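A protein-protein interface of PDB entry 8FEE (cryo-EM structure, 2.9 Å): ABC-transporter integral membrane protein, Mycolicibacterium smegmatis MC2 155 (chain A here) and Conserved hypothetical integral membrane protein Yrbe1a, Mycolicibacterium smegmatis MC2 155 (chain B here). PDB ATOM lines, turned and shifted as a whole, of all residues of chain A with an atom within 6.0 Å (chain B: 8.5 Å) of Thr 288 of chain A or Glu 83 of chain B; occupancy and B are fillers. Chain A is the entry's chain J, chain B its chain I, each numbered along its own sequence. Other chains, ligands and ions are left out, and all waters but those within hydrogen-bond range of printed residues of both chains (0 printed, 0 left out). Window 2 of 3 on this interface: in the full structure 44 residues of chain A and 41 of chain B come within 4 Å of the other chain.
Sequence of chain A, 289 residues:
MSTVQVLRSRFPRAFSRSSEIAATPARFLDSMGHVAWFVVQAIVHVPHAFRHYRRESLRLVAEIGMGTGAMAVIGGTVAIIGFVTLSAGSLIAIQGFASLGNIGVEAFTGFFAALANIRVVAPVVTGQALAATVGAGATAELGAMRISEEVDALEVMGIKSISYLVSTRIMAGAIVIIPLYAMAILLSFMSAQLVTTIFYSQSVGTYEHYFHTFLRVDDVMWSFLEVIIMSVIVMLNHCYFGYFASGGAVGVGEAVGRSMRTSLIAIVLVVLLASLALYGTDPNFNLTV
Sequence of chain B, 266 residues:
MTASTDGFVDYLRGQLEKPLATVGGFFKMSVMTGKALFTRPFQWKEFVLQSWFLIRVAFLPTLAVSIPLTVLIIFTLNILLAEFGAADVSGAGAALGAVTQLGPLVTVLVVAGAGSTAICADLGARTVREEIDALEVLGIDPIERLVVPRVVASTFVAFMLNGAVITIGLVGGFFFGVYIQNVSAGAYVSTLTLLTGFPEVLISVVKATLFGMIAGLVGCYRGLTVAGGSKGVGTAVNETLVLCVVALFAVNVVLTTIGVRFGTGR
Of the printed residues of chain B, Pro 283 of chain A touches Glu 83.
Of the printed residues of chain B, Phe 285 of chain A touches Leu 80 and Glu 83.
Printed residues of chain B within 4 Å of Leu 287 of chain A: Phe 84.
Of chain B, only Glu 83 (3.5 Å) comes within 4 Å of Thr 288 of chain A.
Of the printed residues of chain A, Leu 80 of chain B touches Phe 285 (3.8 Å).
Leu 81 of chain B touches none of the printed residues of chain A.
Of the printed residues of chain A, Glu 83 of chain B touches Pro 283 (3.3 Å), Phe 285 (2.9 Å), Asn 286 (3.6 Å) and Thr 288 (3.5 Å).
Of the printed residues of chain A, Phe 84 of chain B touches Leu 287 (3.5 Å).
The nearest residue of chain B that does not touch Thr 288 of chain A is Phe 84 of chain B (4.7 Å).
The nearest residue of chain A that does not touch Glu 83 of chain B is Leu 287 of chain A (4.6 Å).
Printed residues of chain B that touch a printed residue of chain A: Leu 80, Glu 83 and Phe 84.
Hydrophobic or aromatic side chains of chain B within 4 Å of the printed part of chain A: Leu 80 and Phe 84.
Printed residues of chain A that touch a printed residue of chain B: Pro 283, Phe 285, Asn 286, Leu 287 and Thr 288.
Hydrophobic or aromatic side chains of chain A that line the printed part of chain B: Pro 283, Phe 285 and Leu 287.
Among the printed residues, 6 pairs touch across the chains.
Among the printed residues, no Asp or Glu carboxylate lies within 4 Å of a Lys or Arg side-chain nitrogen of the other chain.
The side-chain carboxylate (OE1) of Glu 83 of chain B sits close to the backbone carbonyl oxygen (O) of Phe 285 of chain A.
Among the printed residues, pairs that only touch across the chains: Pro 283 of chain A with Glu 83 of chain B, Phe 285 of chain A with Leu 80 of chain B, Asn 286 of chain A with Glu 83 of chain B, Leu 287 of chain A with Phe 84 of chain B and Thr 288 of chain A with Glu 83 of chain B.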
ATOM      1  N   PRO A 283     -19.847   6.548  12.551  1.00  0.00           N
ATOM      2  CA  PRO A 283     -20.519   5.346  12.032  1.00  0.00           C
ATOM      3  C   PRO A 283     -20.676   5.325  10.521  1.00  0.00           C
ATOM      4  O   PRO A 283     -21.102   4.292   9.987  1.00  0.00           O
ATOM      5  CB  PRO A 283     -21.882   5.383  12.729  1.00  0.00           C
ATOM      6  CG  PRO A 283     -22.106   6.826  13.008  1.00  0.00           C
ATOM      7  CD  PRO A 283     -20.763   7.411  13.314  1.00  0.00           C
ATOM      8  N   PHE A 285     -22.805   6.635   8.484  1.00  0.00           N
ATOM      9  CA  PHE A 285     -24.182   6.394   8.068  1.00  0.00           C
ATOM     10  C   PHE A 285     -25.054   7.535   8.567  1.00  0.00           C
ATOM     11  O   PHE A 285     -24.976   7.904   9.741  1.00  0.00           O
ATOM     12  CB  PHE A 285     -24.691   5.051   8.603  1.00  0.00           C
ATOM     13  CG  PHE A 285     -26.167   4.850   8.432  1.00  0.00           C
ATOM     14  CD1 PHE A 285     -26.716   4.676   7.175  1.00  0.00           C
ATOM     15  CD2 PHE A 285     -27.007   4.827   9.534  1.00  0.00           C
ATOM     16  CE1 PHE A 285     -28.075   4.492   7.019  1.00  0.00           C
ATOM     17  CE2 PHE A 285     -28.366   4.642   9.385  1.00  0.00           C
ATOM     18  CZ  PHE A 285     -28.901   4.474   8.126  1.00  0.00           C
ATOM     19  N   ASN A 286     -25.869   8.097   7.677  1.00  0.00           N
ATOM     20  CA  ASN A 286     -26.719   9.233   8.014  1.00  0.00           C
ATOM     21  C   ASN A 286     -28.078   9.076   7.350  1.00  0.00           C
ATOM     22  O   ASN A 286     -28.156   8.863   6.138  1.00  0.00           O
ATOM     23  CB  ASN A 286     -26.075  10.555   7.580  1.00  0.00           C
ATOM     24  CG  ASN A 286     -24.776  10.837   8.307  1.00  0.00           C
ATOM     25  OD1 ASN A 286     -23.699  10.465   7.842  1.00  0.00           O
ATOM     26  ND2 ASN A 286     -24.872  11.499   9.453  1.00  0.00           N
ATOM     27  N   LEU A 287     -29.141   9.174   8.147  1.00  0.00           N
ATOM     28  CA  LEU A 287     -30.504   9.200   7.629  1.00  0.00           C
ATOM     29  C   LEU A 287     -31.260  10.457   8.030  1.00  0.00           C
ATOM     30  O   LEU A 287     -31.861  11.113   7.171  1.00  0.00           O
ATOM     31  CB  LEU A 287     -31.275   7.959   8.102  1.00  0.00           C
ATOM     32  CG  LEU A 287     -32.744   7.897   7.680  1.00  0.00           C
ATOM     33  CD1 LEU A 287     -32.882   7.430   6.239  1.00  0.00           C
ATOM     34  CD2 LEU A 287     -33.537   7.006   8.617  1.00  0.00           C
ATOM     35  N   THR A 288     -31.246  10.814   9.312  1.00  0.00           N
ATOM     36  CA  THR A 288     -32.028  11.934   9.808  1.00  0.00           C
ATOM     37  C   THR A 288     -31.272  13.243   9.589  1.00  0.00           C
ATOM     38  O   THR A 288     -30.185  13.274   9.006  1.00  0.00           O
ATOM     39  CB  THR A 288     -32.367  11.734  11.283  1.00  0.00           C
ATOM     40  OG1 THR A 288     -33.118  12.857  11.760  1.00  0.00           O
ATOM     41  CG2 THR A 288     -31.096  11.599  12.104  1.00  0.00           C
ATOM     42  N   VAL A 289     -31.853  14.342  10.061  1.00  0.00           N
ATOM     43  CA  VAL A 289     -31.226  15.647   9.889  1.00  0.00           C
ATOM     44  C   VAL A 289     -30.019  15.767  10.813  1.00  0.00           C
ATOM     45  O   VAL A 289     -29.186  16.660  10.656  1.00  0.00           O
ATOM     46  CB  VAL A 289     -32.217  16.811  10.140  1.00  0.00           C
ATOM     47  CG1 VAL A 289     -33.343  16.801   9.121  1.00  0.00           C
ATOM     48  CG2 VAL A 289     -32.753  16.772  11.539  1.00  0.00           C
ATOM     49  OXT VAL A 289     -29.844  14.976  11.739  1.00  0.00           O
ATOM     50  N   THR B  76     -22.752  -2.921  15.705  1.00  0.00           N
ATOM     51  CA  THR B  76     -23.288  -2.453  14.429  1.00  0.00           C
ATOM     52  C   THR B  76     -24.741  -2.018  14.578  1.00  0.00           C
ATOM     53  O   THR B  76     -25.137  -0.946  14.100  1.00  0.00           O
ATOM     54  CB  THR B  76     -23.159  -3.549  13.371  1.00  0.00           C
ATOM     55  OG1 THR B  76     -21.773  -3.821  13.131  1.00  0.00           O
ATOM     56  CG2 THR B  76     -23.814  -3.117  12.069  1.00  0.00           C
ATOM     57  N   LEU B  77     -25.547  -2.832  15.265  1.00  0.00           N
ATOM     58  CA  LEU B  77     -26.962  -2.518  15.427  1.00  0.00           C
ATOM     59  C   LEU B  77     -27.147  -1.226  16.205  1.00  0.00           C
ATOM     60  O   LEU B  77     -27.966  -0.380  15.830  1.00  0.00           O
ATOM     61  CB  LEU B  77     -27.677  -3.674  16.125  1.00  0.00           C
ATOM     62  CG  LEU B  77     -29.205  -3.639  16.105  1.00  0.00           C
ATOM     63  CD1 LEU B  77     -29.722  -3.786  14.684  1.00  0.00           C
ATOM     64  CD2 LEU B  77     -29.770  -4.725  17.001  1.00  0.00           C
ATOM     65  N   ASN B  78     -26.386  -1.050  17.288  1.00  0.00           N
ATOM     66  CA  ASN B  78     -26.527   0.145  18.108  1.00  0.00           C
ATOM     67  C   ASN B  78     -26.131   1.397  17.340  1.00  0.00           C
ATOM     68  O   ASN B  78     -26.831   2.413  17.416  1.00  0.00           O
ATOM     69  CB  ASN B  78     -25.691   0.015  19.380  1.00  0.00           C
ATOM     70  CG  ASN B  78     -26.364  -0.835  20.431  1.00  0.00           C
ATOM     71  OD1 ASN B  78     -27.549  -1.139  20.331  1.00  0.00           O
ATOM     72  ND2 ASN B  78     -25.609  -1.221  21.452  1.00  0.00           N
ATOM     73  N   ILE B  79     -25.019   1.357  16.596  1.00  0.00           N
ATOM     74  CA  ILE B  79     -24.615   2.565  15.877  1.00  0.00           C
ATOM     75  C   ILE B  79     -25.620   2.895  14.774  1.00  0.00           C
ATOM     76  O   ILE B  79     -25.997   4.064  14.594  1.00  0.00           O
ATOM     77  CB  ILE B  79     -23.168   2.454  15.350  1.00  0.00           C
ATOM     78  CG1 ILE B  79     -23.014   1.387  14.265  1.00  0.00           C
ATOM     79  CG2 ILE B  79     -22.198   2.201  16.494  1.00  0.00           C
ATOM     80  CD1 ILE B  79     -21.679   1.428  13.559  1.00  0.00           C
ATOM     81  N   LEU B  80     -26.094   1.879  14.040  1.00  0.00           N
ATOM     82  CA  LEU B  80     -27.053   2.147  12.972  1.00  0.00           C
ATOM     83  C   LEU B  80     -28.371   2.674  13.526  1.00  0.00           C
ATOM     84  O   LEU B  80     -28.979   3.573  12.936  1.00  0.00           O
ATOM     85  CB  LEU B  80     -27.280   0.891  12.133  1.00  0.00           C
ATOM     86  CG  LEU B  80     -26.044   0.376  11.392  1.00  0.00           C
ATOM     87  CD1 LEU B  80     -26.393  -0.815  10.515  1.00  0.00           C
ATOM     88  CD2 LEU B  80     -25.393   1.488  10.583  1.00  0.00           C
ATOM     89  N   LEU B  81     -28.828   2.133  14.659  1.00  0.00           N
ATOM     90  CA  LEU B  81     -30.079   2.608  15.242  1.00  0.00           C
ATOM     91  C   LEU B  81     -29.930   4.013  15.811  1.00  0.00           C
ATOM     92  O   LEU B  81     -30.847   4.833  15.692  1.00  0.00           O
ATOM     93  CB  LEU B  81     -30.567   1.634  16.312  1.00  0.00           C
ATOM     94  CG  LEU B  81     -31.177   0.342  15.766  1.00  0.00           C
ATOM     95  CD1 LEU B  81     -31.808  -0.463  16.880  1.00  0.00           C
ATOM     96  CD2 LEU B  81     -32.195   0.643  14.678  1.00  0.00           C
ATOM     97  N   ALA B  82     -28.793   4.305  16.452  1.00  0.00           N
ATOM     98  CA  ALA B  82     -28.575   5.643  16.992  1.00  0.00           C
ATOM     99  C   ALA B  82     -28.550   6.682  15.880  1.00  0.00           C
ATOM    100  O   ALA B  82     -29.086   7.785  16.041  1.00  0.00           O
ATOM    101  CB  ALA B  82     -27.276   5.681  17.796  1.00  0.00           C
ATOM    102  N   GLU B  83     -27.923   6.353  14.746  1.00  0.00           N
ATOM    103  CA  GLU B  83     -28.014   7.235  13.585  1.00  0.00           C
ATOM    104  C   GLU B  83     -29.445   7.328  13.070  1.00  0.00           C
ATOM    105  O   GLU B  83     -29.899   8.404  12.662  1.00  0.00           O
ATOM    106  CB  GLU B  83     -27.073   6.757  12.484  1.00  0.00           C
ATOM    107  CG  GLU B  83     -25.628   7.087  12.761  1.00  0.00           C
ATOM    108  CD  GLU B  83     -25.371   8.581  12.804  1.00  0.00           C
ATOM    109  OE1 GLU B  83     -26.006   9.320  12.023  1.00  0.00           O
ATOM    110  OE2 GLU B  83     -24.537   9.020  13.625  1.00  0.00           O
ATOM    111  N   PHE B  84     -30.167   6.204  13.070  1.00  0.00           N
ATOM    112  CA  PHE B  84     -31.584   6.213  12.724  1.00  0.00           C
ATOM    113  C   PHE B  84     -32.396   7.044  13.707  1.00  0.00           C
ATOM    114  O   PHE B  84     -33.413   7.636  13.330  1.00  0.00           O
ATOM    115  CB  PHE B  84     -32.107   4.775  12.687  1.00  0.00           C
ATOM    116  CG  PHE B  84     -33.244   4.556  11.733  1.00  0.00           C
ATOM    117  CD1 PHE B  84     -34.522   4.989  12.043  1.00  0.00           C
ATOM    118  CD2 PHE B  84     -33.040   3.890  10.535  1.00  0.00           C
ATOM    119  CE1 PHE B  84     -35.571   4.780  11.170  1.00  0.00           C
ATOM    120  CE2 PHE B  84     -34.085   3.673   9.660  1.00  0.00           C
ATOM    121  CZ  PHE B  84     -35.352   4.121   9.977  1.00  0.00           C
ATOM    122  N   GLY B  85     -31.963   7.108  14.965  1.00  0.00           N
ATOM    123  CA  GLY B  85     -32.660   7.826  16.003  1.00  0.00           C
ATOM    124  C   GLY B  85     -33.466   6.949  16.938  1.00  0.00           C
ATOM    125  O   GLY B  85     -33.780   7.380  18.053  1.00  0.00           O
ATOM    126  N   ALA B  86     -33.800   5.732  16.517  1.00  0.00           N
ATOM    127  CA  ALA B  86     -34.612   4.824  17.325  1.00  0.00           C
ATOM    128  C   ALA B  86     -33.711   3.772  17.969  1.00  0.00           C
ATOM    129  O   ALA B  86     -33.670   2.606  17.576  1.00  0.00           O
ATOM    130  CB  ALA B  86     -35.705   4.188  16.473  1.00  0.00           C
ATOM    131  N   ALA B  87     -32.985   4.215  18.990  1.00  0.00           N
ATOM    132  CA  ALA B  87     -32.070   3.355  19.725  1.00  0.00           C
ATOM    133  C   ALA B  87     -32.715   2.698  20.936  1.00  0.00           C
ATOM    134  O   ALA B  87     -32.024   1.999  21.683  1.00  0.00           O
ATOM    135  CB  ALA B  87     -30.839   4.150  20.168  1.00  0.00           C
